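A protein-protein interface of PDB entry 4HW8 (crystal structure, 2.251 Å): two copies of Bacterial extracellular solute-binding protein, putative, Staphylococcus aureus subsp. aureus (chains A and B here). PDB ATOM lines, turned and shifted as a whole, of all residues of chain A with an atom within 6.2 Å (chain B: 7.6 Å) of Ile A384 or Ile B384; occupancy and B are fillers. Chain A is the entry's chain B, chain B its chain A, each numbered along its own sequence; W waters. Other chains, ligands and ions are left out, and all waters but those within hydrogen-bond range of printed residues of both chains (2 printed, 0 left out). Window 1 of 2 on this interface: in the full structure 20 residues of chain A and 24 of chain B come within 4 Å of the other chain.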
ATOM      1  N   ALA A 191      12.749   7.629 -15.566  1.00  0.00           N
ATOM      2  CA  ALA A 191      11.705   6.786 -16.118  1.00  0.00           C
ATOM      3  C   ALA A 191      12.090   5.315 -16.349  1.00  0.00           C
ATOM      4  O   ALA A 191      11.218   4.524 -16.715  1.00  0.00           O
ATOM      5  CB  ALA A 191      11.168   7.413 -17.439  1.00  0.00           C
ATOM      6  N   LYS A 192      13.366   4.952 -16.163  1.00  0.00           N
ATOM      7  CA  LYS A 192      13.778   3.551 -16.306  1.00  0.00           C
ATOM      8  C   LYS A 192      13.617   2.820 -14.941  1.00  0.00           C
ATOM      9  O   LYS A 192      13.826   1.627 -14.868  1.00  0.00           O
ATOM     10  CB  LYS A 192      15.254   3.396 -16.639  1.00  0.00           C
ATOM     11  CG  LYS A 192      15.913   4.310 -17.608  1.00  0.00           C
ATOM     12  CD  LYS A 192      16.142   3.771 -18.971  1.00  0.00           C
ATOM     13  CE  LYS A 192      17.465   4.328 -19.511  1.00  0.00           C
ATOM     14  NZ  LYS A 192      17.739   5.736 -19.064  1.00  0.00           N
ATOM     15  N   MET A 379      10.136  -5.090 -13.534  1.00  0.00           N
ATOM     16  CA  MET A 379       9.520  -3.833 -13.954  1.00  0.00           C
ATOM     17  C   MET A 379      10.597  -2.826 -14.379  1.00  0.00           C
ATOM     18  O   MET A 379      10.380  -2.013 -15.294  1.00  0.00           O
ATOM     19  CB  MET A 379       8.627  -3.254 -12.866  1.00  0.00           C
ATOM     20  CG  MET A 379       7.308  -4.000 -12.738  1.00  0.00           C
ATOM     21  SD  MET A 379       6.380  -3.989 -14.289  1.00  0.00           S
ATOM     22  CE  MET A 379       5.947  -2.241 -14.437  1.00  0.00           C
ATOM     23  N   GLY A 380      11.756  -2.893 -13.734  1.00  0.00           N
ATOM     24  CA  GLY A 380      12.887  -2.043 -14.111  1.00  0.00           C
ATOM     25  C   GLY A 380      13.326  -2.426 -15.512  1.00  0.00           C
ATOM     26  O   GLY A 380      13.552  -1.557 -16.355  1.00  0.00           O
ATOM     27  N   ASN A 381      13.427  -3.731 -15.782  1.00  0.00           N
ATOM     28  CA  ASN A 381      13.846  -4.170 -17.102  1.00  0.00           C
ATOM     29  C   ASN A 381      12.807  -3.744 -18.146  1.00  0.00           C
ATOM     30  O   ASN A 381      13.149  -3.269 -19.228  1.00  0.00           O
ATOM     31  CB  ASN A 381      14.070  -5.688 -17.148  1.00  0.00           C
ATOM     32  CG  ASN A 381      15.326  -6.145 -16.376  1.00  0.00           C
ATOM     33  OD1 ASN A 381      16.008  -5.357 -15.709  1.00  0.00           O
ATOM     34  ND2 ASN A 381      15.628  -7.428 -16.481  1.00  0.00           N
ATOM     35  N   ALA A 382      11.531  -3.906 -17.813  1.00  0.00           N
ATOM     36  CA  ALA A 382      10.475  -3.532 -18.744  1.00  0.00           C
ATOM     37  C   ALA A 382      10.625  -2.066 -19.093  1.00  0.00           C
ATOM     38  O   ALA A 382      10.559  -1.693 -20.263  1.00  0.00           O
ATOM     39  CB  ALA A 382       9.117  -3.798 -18.145  1.00  0.00           C
ATOM     40  N   SER A 383      10.857  -1.245 -18.076  1.00  0.00           N
ATOM     41  CA  SER A 383      11.014   0.202 -18.253  1.00  0.00           C
ATOM     42  C   SER A 383      12.221   0.533 -19.149  1.00  0.00           C
ATOM     43  O   SER A 383      12.126   1.380 -20.044  1.00  0.00           O
ATOM     44  CB  SER A 383      11.137   0.882 -16.892  1.00  0.00           C
ATOM     45  OG  SER A 383      10.019   0.558 -16.059  1.00  0.00           O
ATOM     46  N   ILE A 384      13.344  -0.152 -18.924  1.00  0.00           N
ATOM     47  CA  ILE A 384      14.510   0.014 -19.792  1.00  0.00           C
ATOM     48  C   ILE A 384      14.118  -0.338 -21.231  1.00  0.00           C
ATOM     49  O   ILE A 384      14.397   0.427 -22.167  1.00  0.00           O
ATOM     50  CB  ILE A 384      15.708  -0.856 -19.328  1.00  0.00           C
ATOM     51  CG1 ILE A 384      16.232  -0.317 -17.977  1.00  0.00           C
ATOM     52  CG2 ILE A 384      16.830  -0.843 -20.407  1.00  0.00           C
ATOM     53  CD1 ILE A 384      17.151  -1.235 -17.241  1.00  0.00           C
ATOM     54  N   PHE A 385      13.433  -1.466 -21.415  1.00  0.00           N
ATOM     55  CA  PHE A 385      13.043  -1.896 -22.784  1.00  0.00           C
ATOM     56  C   PHE A 385      12.101  -0.884 -23.438  1.00  0.00           C
ATOM     57  O   PHE A 385      12.280  -0.528 -24.585  1.00  0.00           O
ATOM     58  CB  PHE A 385      12.424  -3.296 -22.801  1.00  0.00           C
ATOM     59  CG  PHE A 385      13.376  -4.404 -22.420  1.00  0.00           C
ATOM     60  CD1 PHE A 385      14.613  -4.521 -23.029  1.00  0.00           C
ATOM     61  CD2 PHE A 385      12.998  -5.379 -21.503  1.00  0.00           C
ATOM     62  CE1 PHE A 385      15.480  -5.559 -22.697  1.00  0.00           C
ATOM     63  CE2 PHE A 385      13.857  -6.416 -21.175  1.00  0.00           C
ATOM     64  CZ  PHE A 385      15.097  -6.502 -21.780  1.00  0.00           C
ATOM     65  N   ILE A 386      11.126  -0.396 -22.680  1.00  0.00           N
ATOM     66  CA  ILE A 386      10.201   0.622 -23.166  1.00  0.00           C
ATOM     67  C   ILE A 386      10.963   1.859 -23.655  1.00  0.00           C
ATOM     68  O   ILE A 386      10.681   2.370 -24.727  1.00  0.00           O
ATOM     69  CB  ILE A 386       9.171   0.975 -22.059  1.00  0.00           C
ATOM     70  CG1 ILE A 386       8.189  -0.197 -21.892  1.00  0.00           C
ATOM     71  CG2 ILE A 386       8.403   2.293 -22.372  1.00  0.00           C
ATOM     72  CD1 ILE A 386       7.321  -0.117 -20.617  1.00  0.00           C
ATOM     73  N   SER A 387      11.955   2.306 -22.889  1.00  0.00           N
ATOM     74  CA  SER A 387      12.772   3.456 -23.273  1.00  0.00           C
ATOM     75  C   SER A 387      13.563   3.185 -24.538  1.00  0.00           C
ATOM     76  O   SER A 387      13.956   4.107 -25.216  1.00  0.00           O
ATOM     77  CB  SER A 387      13.777   3.831 -22.169  1.00  0.00           C
ATOM     78  OG  SER A 387      14.882   2.929 -22.113  1.00  0.00           O
ATOM     79  N   ASN A 388      13.816   1.916 -24.832  1.00  0.00           N
ATOM     80  CA  ASN A 388      14.594   1.528 -25.994  1.00  0.00           C
ATOM     81  C   ASN A 388      13.712   1.182 -27.202  1.00  0.00           C
ATOM     82  O   ASN A 388      14.199   0.691 -28.212  1.00  0.00           O
ATOM     83  CB  ASN A 388      15.491   0.336 -25.622  1.00  0.00           C
ATOM     84  CG  ASN A 388      16.463  -0.041 -26.727  1.00  0.00           C
ATOM     85  OD1 ASN A 388      17.169   0.809 -27.266  1.00  0.00           O
ATOM     86  ND2 ASN A 388      16.521  -1.328 -27.049  1.00  0.00           N
ATOM     87  N   GLY A 389      12.406   1.398 -27.082  1.00  0.00           N
ATOM     88  CA  GLY A 389      11.497   1.189 -28.212  1.00  0.00           C
ATOM     89  C   GLY A 389      10.727  -0.114 -28.273  1.00  0.00           C
ATOM     90  O   GLY A 389       9.984  -0.330 -29.212  1.00  0.00           O
ATOM     91  N   ALA B 191      24.196 -12.389 -15.270  1.00  0.00           N
ATOM     92  CA  ALA B 191      24.828 -11.768 -16.423  1.00  0.00           C
ATOM     93  C   ALA B 191      24.258 -10.413 -16.826  1.00  0.00           C
ATOM     94  O   ALA B 191      24.812  -9.761 -17.705  1.00  0.00           O
ATOM     95  CB  ALA B 191      24.788 -12.731 -17.599  1.00  0.00           C
ATOM     96  N   LYS B 192      23.143 -10.015 -16.230  1.00  0.00           N
ATOM     97  CA  LYS B 192      22.545  -8.689 -16.472  1.00  0.00           C
ATOM     98  C   LYS B 192      23.272  -7.608 -15.676  1.00  0.00           C
ATOM     99  O   LYS B 192      23.100  -6.427 -15.952  1.00  0.00           O
ATOM    100  CB  LYS B 192      21.124  -8.635 -15.961  1.00  0.00           C
ATOM    101  CG  LYS B 192      19.984  -8.761 -16.919  1.00  0.00           C
ATOM    102  CD  LYS B 192      19.828 -10.067 -17.550  1.00  0.00           C
ATOM    103  CE  LYS B 192      18.358 -10.288 -17.852  1.00  0.00           C
ATOM    104  NZ  LYS B 192      17.704 -10.666 -16.597  1.00  0.00           N
ATOM    105  N   ASN B 193      24.008  -8.017 -14.641  1.00  0.00           N
ATOM    106  CA  ASN B 193      24.709  -7.076 -13.767  1.00  0.00           C
ATOM    107  C   ASN B 193      26.198  -7.051 -14.081  1.00  0.00           C
ATOM    108  O   ASN B 193      26.854  -8.079 -14.064  1.00  0.00           O
ATOM    109  CB  ASN B 193      24.473  -7.443 -12.288  1.00  0.00           C
ATOM    110  CG  ASN B 193      25.147  -6.477 -11.320  1.00  0.00           C
ATOM    111  OD1 ASN B 193      26.023  -5.678 -11.700  1.00  0.00           O
ATOM    112  ND2 ASN B 193      24.755  -6.555 -10.056  1.00  0.00           N
ATOM    113  N   ASN B 197      29.130 -10.045 -14.500  1.00  0.00           N
ATOM    114  CA  ASN B 197      29.575 -10.483 -15.820  1.00  0.00           C
ATOM    115  C   ASN B 197      30.968  -9.996 -16.215  1.00  0.00           C
ATOM    116  O   ASN B 197      31.528 -10.470 -17.202  1.00  0.00           O
ATOM    117  CB  ASN B 197      28.537 -10.138 -16.883  1.00  0.00           C
ATOM    118  CG  ASN B 197      28.427  -8.654 -17.152  1.00  0.00           C
ATOM    119  OD1 ASN B 197      29.375  -7.891 -16.922  1.00  0.00           O
ATOM    120  ND2 ASN B 197      27.271  -8.238 -17.680  1.00  0.00           N
ATOM    121  N   GLN B 236      26.168 -13.471 -25.278  1.00  0.00           N
ATOM    122  CA  GLN B 236      24.879 -13.545 -25.968  1.00  0.00           C
ATOM    123  C   GLN B 236      24.611 -14.961 -26.463  1.00  0.00           C
ATOM    124  O   GLN B 236      23.475 -15.422 -26.428  1.00  0.00           O
ATOM    125  CB  GLN B 236      24.815 -12.582 -27.144  1.00  0.00           C
ATOM    126  CG  GLN B 236      23.419 -12.414 -27.644  1.00  0.00           C
ATOM    127  CD  GLN B 236      23.285 -11.212 -28.533  1.00  0.00           C
ATOM    128  OE1 GLN B 236      23.658 -11.249 -29.708  1.00  0.00           O
ATOM    129  NE2 GLN B 236      22.732 -10.129 -27.980  1.00  0.00           N
ATOM    130  N   TYR B 239      23.093 -17.020 -23.850  1.00  0.00           N
ATOM    131  CA  TYR B 239      21.652 -16.777 -23.778  1.00  0.00           C
ATOM    132  C   TYR B 239      20.944 -17.489 -24.939  1.00  0.00           C
ATOM    133  O   TYR B 239      19.891 -18.089 -24.749  1.00  0.00           O
ATOM    134  CB  TYR B 239      21.308 -15.281 -23.811  1.00  0.00           C
ATOM    135  CG  TYR B 239      21.467 -14.575 -22.490  1.00  0.00           C
ATOM    136  CD1 TYR B 239      20.509 -14.722 -21.493  1.00  0.00           C
ATOM    137  CD2 TYR B 239      22.553 -13.737 -22.234  1.00  0.00           C
ATOM    138  CE1 TYR B 239      20.642 -14.098 -20.273  1.00  0.00           C
ATOM    139  CE2 TYR B 239      22.670 -13.072 -21.012  1.00  0.00           C
ATOM    140  CZ  TYR B 239      21.707 -13.270 -20.041  1.00  0.00           C
ATOM    141  OH  TYR B 239      21.791 -12.634 -18.826  1.00  0.00           O
ATOM    142  N   LYS B 246      16.741 -15.646 -18.976  1.00  0.00           N
ATOM    143  CA  LYS B 246      16.525 -14.203 -19.041  1.00  0.00           C
ATOM    144  C   LYS B 246      15.688 -13.650 -17.898  1.00  0.00           C
ATOM    145  O   LYS B 246      15.909 -12.535 -17.465  1.00  0.00           O
ATOM    146  CB  LYS B 246      15.847 -13.829 -20.361  1.00  0.00           C
ATOM    147  CG  LYS B 246      16.666 -14.132 -21.589  1.00  0.00           C
ATOM    148  CD  LYS B 246      15.842 -13.883 -22.851  1.00  0.00           C
ATOM    149  CE  LYS B 246      16.650 -14.201 -24.121  1.00  0.00           C
ATOM    150  NZ  LYS B 246      17.032 -15.637 -24.187  1.00  0.00           N
ATOM    151  N   GLU B 377      25.460   1.821 -14.294  1.00  0.00           N
ATOM    152  CA  GLU B 377      24.155   1.736 -14.894  1.00  0.00           C
ATOM    153  C   GLU B 377      24.197   1.558 -16.419  1.00  0.00           C
ATOM    154  O   GLU B 377      23.497   0.694 -16.955  1.00  0.00           O
ATOM    155  CB  GLU B 377      23.235   2.900 -14.436  1.00  0.00           C
ATOM    156  CG  GLU B 377      21.828   2.781 -15.020  1.00  0.00           C
ATOM    157  CD  GLU B 377      20.771   3.656 -14.336  1.00  0.00           C
ATOM    158  OE1 GLU B 377      20.959   4.085 -13.186  1.00  0.00           O
ATOM    159  OE2 GLU B 377      19.725   3.896 -14.966  1.00  0.00           O
ATOM    160  N   PRO B 378      24.994   2.365 -17.130  1.00  0.00           N
ATOM    161  CA  PRO B 378      25.047   2.144 -18.569  1.00  0.00           C
ATOM    162  C   PRO B 378      25.503   0.728 -18.947  1.00  0.00           C
ATOM    163  O   PRO B 378      24.980   0.166 -19.906  1.00  0.00           O
ATOM    164  CB  PRO B 378      26.054   3.184 -19.044  1.00  0.00           C
ATOM    165  CG  PRO B 378      25.946   4.264 -18.067  1.00  0.00           C
ATOM    166  CD  PRO B 378      25.697   3.593 -16.749  1.00  0.00           C
ATOM    167  N   MET B 379      26.473   0.169 -18.229  1.00  0.00           N
ATOM    168  CA  MET B 379      26.909  -1.207 -18.525  1.00  0.00           C
ATOM    169  C   MET B 379      25.852  -2.219 -18.113  1.00  0.00           C
ATOM    170  O   MET B 379      25.704  -3.262 -18.746  1.00  0.00           O
ATOM    171  CB  MET B 379      28.257  -1.520 -17.882  1.00  0.00           C
ATOM    172  CG  MET B 379      29.429  -0.796 -18.542  1.00  0.00           C
ATOM    173  SD  MET B 379      29.713  -1.329 -20.235  1.00  0.00           S
ATOM    174  CE  MET B 379      30.131  -3.081 -19.979  1.00  0.00           C
ATOM    175  N   GLY B 380      25.099  -1.914 -17.059  1.00  0.00           N
ATOM    176  CA  GLY B 380      23.994  -2.777 -16.663  1.00  0.00           C
ATOM    177  C   GLY B 380      22.953  -2.774 -17.782  1.00  0.00           C
ATOM    178  O   GLY B 380      22.445  -3.821 -18.178  1.00  0.00           O
ATOM    179  N   ASN B 381      22.646  -1.587 -18.293  1.00  0.00           N
ATOM    180  CA  ASN B 381      21.673  -1.448 -19.364  1.00  0.00           C
ATOM    181  C   ASN B 381      22.135  -2.219 -20.599  1.00  0.00           C
ATOM    182  O   ASN B 381      21.359  -2.992 -21.183  1.00  0.00           O
ATOM    183  CB  ASN B 381      21.425   0.014 -19.703  1.00  0.00           C
ATOM    184  CG  ASN B 381      20.536   0.742 -18.674  1.00  0.00           C
ATOM    185  OD1 ASN B 381      20.213   0.224 -17.592  1.00  0.00           O
ATOM    186  ND2 ASN B 381      20.121   1.964 -19.038  1.00  0.00           N
ATOM    187  N   ALA B 382      23.399  -2.042 -20.985  1.00  0.00           N
ATOM    188  CA  ALA B 382      23.925  -2.757 -22.147  1.00  0.00           C
ATOM    189  C   ALA B 382      23.817  -4.282 -21.928  1.00  0.00           C
ATOM    190  O   ALA B 382      23.462  -5.030 -22.857  1.00  0.00           O
ATOM    191  CB  ALA B 382      25.327  -2.354 -22.421  1.00  0.00           C
ATOM    192  N   SER B 383      24.087  -4.740 -20.702  1.00  0.00           N
ATOM    193  CA  SER B 383      24.021  -6.178 -20.395  1.00  0.00           C
ATOM    194  C   SER B 383      22.579  -6.675 -20.554  1.00  0.00           C
ATOM    195  O   SER B 383      22.342  -7.737 -21.121  1.00  0.00           O
ATOM    196  CB  SER B 383      24.545  -6.451 -18.993  1.00  0.00           C
ATOM    197  OG  SER B 383      25.873  -5.949 -18.827  1.00  0.00           O
ATOM    198  N   ILE B 384      21.622  -5.875 -20.086  1.00  0.00           N
ATOM    199  CA  ILE B 384      20.226  -6.199 -20.233  1.00  0.00           C
ATOM    200  C   ILE B 384      19.891  -6.318 -21.722  1.00  0.00           C
ATOM    201  O   ILE B 384      19.305  -7.319 -22.150  1.00  0.00           O
ATOM    202  CB  ILE B 384      19.328  -5.160 -19.523  1.00  0.00           C
ATOM    203  CG1 ILE B 384      19.555  -5.246 -18.006  1.00  0.00           C
ATOM    204  CG2 ILE B 384      17.849  -5.424 -19.824  1.00  0.00           C
ATOM    205  CD1 ILE B 384      19.054  -4.025 -17.203  1.00  0.00           C
ATOM    206  N   PHE B 385      20.295  -5.325 -22.514  1.00  0.00           N
ATOM    207  CA  PHE B 385      20.022  -5.342 -23.950  1.00  0.00           C
ATOM    208  C   PHE B 385      20.635  -6.561 -24.628  1.00  0.00           C
ATOM    209  O   PHE B 385      20.014  -7.207 -25.450  1.00  0.00           O
ATOM    210  CB  PHE B 385      20.495  -4.057 -24.625  1.00  0.00           C
ATOM    211  CG  PHE B 385      19.729  -2.798 -24.197  1.00  0.00           C
ATOM    212  CD1 PHE B 385      18.343  -2.781 -24.159  1.00  0.00           C
ATOM    213  CD2 PHE B 385      20.406  -1.616 -23.906  1.00  0.00           C
ATOM    214  CE1 PHE B 385      17.661  -1.621 -23.786  1.00  0.00           C
ATOM    215  CE2 PHE B 385      19.716  -0.464 -23.539  1.00  0.00           C
ATOM    216  CZ  PHE B 385      18.349  -0.471 -23.492  1.00  0.00           C
ATOM    217  N   ILE B 386      21.858  -6.880 -24.259  1.00  0.00           N
ATOM    218  CA  ILE B 386      22.536  -8.044 -24.790  1.00  0.00           C
ATOM    219  C   ILE B 386      21.737  -9.314 -24.463  1.00  0.00           C
ATOM    220  O   ILE B 386      21.565 -10.195 -25.329  1.00  0.00           O
ATOM    221  CB  ILE B 386      23.981  -8.089 -24.264  1.00  0.00           C
ATOM    222  CG1 ILE B 386      24.812  -7.040 -25.039  1.00  0.00           C
ATOM    223  CG2 ILE B 386      24.578  -9.513 -24.376  1.00  0.00           C
ATOM    224  CD1 ILE B 386      26.179  -6.676 -24.384  1.00  0.00           C
ATOM    225  N   SER B 387      21.204  -9.388 -23.248  1.00  0.00           N
ATOM    226  CA  SER B 387      20.404 -10.544 -22.849  1.00  0.00           C
ATOM    227  C   SER B 387      19.142 -10.622 -23.727  1.00  0.00           C
ATOM    228  O   SER B 387      18.663 -11.696 -24.041  1.00  0.00           O
ATOM    229  CB  SER B 387      20.035 -10.488 -21.349  1.00  0.00           C
ATOM    230  OG  SER B 387      19.033  -9.519 -21.059  1.00  0.00           O
ATOM    231  N   ASN B 388      18.644  -9.463 -24.138  1.00  0.00           N
ATOM    232  CA  ASN B 388      17.425  -9.351 -24.963  1.00  0.00           C
ATOM    233  C   ASN B 388      17.679  -9.498 -26.471  1.00  0.00           C
ATOM    234  O   ASN B 388      16.751  -9.460 -27.268  1.00  0.00           O
ATOM    235  CB  ASN B 388      16.776  -7.995 -24.666  1.00  0.00           C
ATOM    236  CG  ASN B 388      15.450  -7.811 -25.336  1.00  0.00           C
ATOM    237  OD1 ASN B 388      14.593  -8.684 -25.300  1.00  0.00           O
ATOM    238  ND2 ASN B 388      15.246  -6.636 -25.901  1.00  0.00           N
ATOM    239  N   GLY B 389      18.934  -9.652 -26.870  1.00  0.00           N
ATOM    240  CA  GLY B 389      19.250  -9.862 -28.285  1.00  0.00           C
ATOM    241  C   GLY B 389      19.853  -8.682 -29.029  1.00  0.00           C
ATOM    242  O   GLY B 389      20.094  -8.774 -30.219  1.00  0.00           O
ATOM    243  N   LYS B 390      20.123  -7.579 -28.349  1.00  0.00           N
ATOM    244  CA  LYS B 390      20.694  -6.445 -29.047  1.00  0.00           C
ATOM    245  C   LYS B 390      22.118  -6.796 -29.503  1.00  0.00           C
ATOM    246  O   LYS B 390      22.845  -7.510 -28.806  1.00  0.00           O
ATOM    247  CB  LYS B 390      20.677  -5.163 -28.173  1.00  0.00           C
ATOM    248  CG  LYS B 390      21.215  -3.912 -28.923  1.00  0.00           C
ATOM    249  CD  LYS B 390      21.136  -2.564 -28.151  1.00  0.00           C
ATOM    250  CE  LYS B 390      19.710  -1.980 -28.047  1.00  0.00           C
ATOM    251  NZ  LYS B 390      19.039  -1.710 -29.390  1.00  0.00           N
ATOM    252  N   ALA B 395      25.367  -2.277 -28.410  1.00  0.00           N
ATOM    253  CA  ALA B 395      25.025  -2.151 -27.012  1.00  0.00           C
ATOM    254  C   ALA B 395      26.160  -1.472 -26.267  1.00  0.00           C
ATOM    255  O   ALA B 395      25.948  -0.472 -25.593  1.00  0.00           O
ATOM    256  CB  ALA B 395      24.713  -3.522 -26.430  1.00  0.00           C
HETATM  257  O   HOH W   1      14.698  -3.216 -26.330  1.00  0.00           O
HETATM  258  O   HOH W   2      20.162   4.800 -17.726  1.00  0.00           O
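Of the 13 printed residues of chain A, 5 touch a printed residue of chain B.
Printed residues of chain A that touch a printed residue of chain B: Lys A192, Asn A381, Ile A384, Phe A385 and Asn A388.
Hydrophobic or aromatic side chains of chain B within 4 Å of the printed part of chain A: Ile B384 and Phe B385.
Among the printed residues, no Asp or Glu carboxylate lies within 4 Å of a Lys or Arg side-chain nitrogen of the other chain.
NZ of Lys B390 sits close to ND2 of Asn A388 (3.5 Å).
Asn A381 touches Ile B384, and with the chains exchanged Ile A384 touches Asn B381.
Ile A384 touches its own counterpart, Ile B384.
Ile A384 touches Phe B385, and with the chains exchanged Phe A385 touches Ile B384.
Phe A385 touches Asn B388, and with the chains exchanged Asn A388 touches Phe B385.
13 positions are printed for both chains.
Of the 10 pairs that touch across the chains among the printed residues, 9 have their exchanged pair printed and touching as well.
Of chain B, only Asn B381, Ile B384 and Phe B385 come within 4 Å of Ile A384.
Of the printed residues of chain B, Asn A388 touches Phe B385 (3.5 Å) and Lys B390 (3.4 Å).
Gln B236 touches none of the printed residues of chain A.
Printed residues of chain A within 4 Å of Asn B381: Lys A192 and Ile A384.
Of chain A, only Asn A381 (3.6 Å), Ile A384 (3.4 Å) and Phe A385 (3.5 Å) come within 4 Å of Ile B384.
Of the printed residues of chain A, Asn B388 touches Phe A385 (3.4 Å).
Of the printed residues of chain A, Lys B390 touches Asn A388.
The nearest residue of chain A that does not touch Ile B384 is Gly A380 (6.1 Å).
Among the printed residues, pairs that only touch across the chains: Lys A192 with Asn B381 (3.6 Å), Asn A381 with Lys B192 (3.8 Å), Asn A381 with Ile B384 (3.6 Å), Ile A384 with Asn B381 (3.4 Å), Ile A384 with Ile B384 (3.4 Å), Ile A384 with Phe B385 (3.5 Å), Phe A385 with Ile B384 (3.5 Å), Phe A385 with Asn B388 (3.4 Å) and Asn A388 with Phe B385 (3.5 Å).
NZ of Lys B192 lies within hydrogen-bond range of O of Lys B246, 2.7 Å away.
The side-chain amide nitrogen (NE2) of Gln B236 is in hydrogen-bond range of the backbone carbonyl oxygen (O) of Lys B390 (2.7 Å).
The backbone carbonyl oxygen (O) of Glu B377 sits close to the side-chain amide oxygen (OD1) of Asn B381.
O of Ile B384 lies within hydrogen-bond range of OG of Ser B387 (2.5 Å).
O of Phe B385 lies within hydrogen-bond range of N of Lys B390, 2.9 Å away.
O of Ile A384 is in hydrogen-bond range of OG of Ser A387, 2.5 Å away.
Water W1 bridges ND2 of Asn A388 (2.7 Å) and ND2 of Asn B388 (3.5 Å).
Water W2 lies within hydrogen-bond range of NZ of Lys A192 (2.9 Å), OE2 of Glu B377 (2.9 Å) and ND2 of Asn B381 (3.1 Å).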
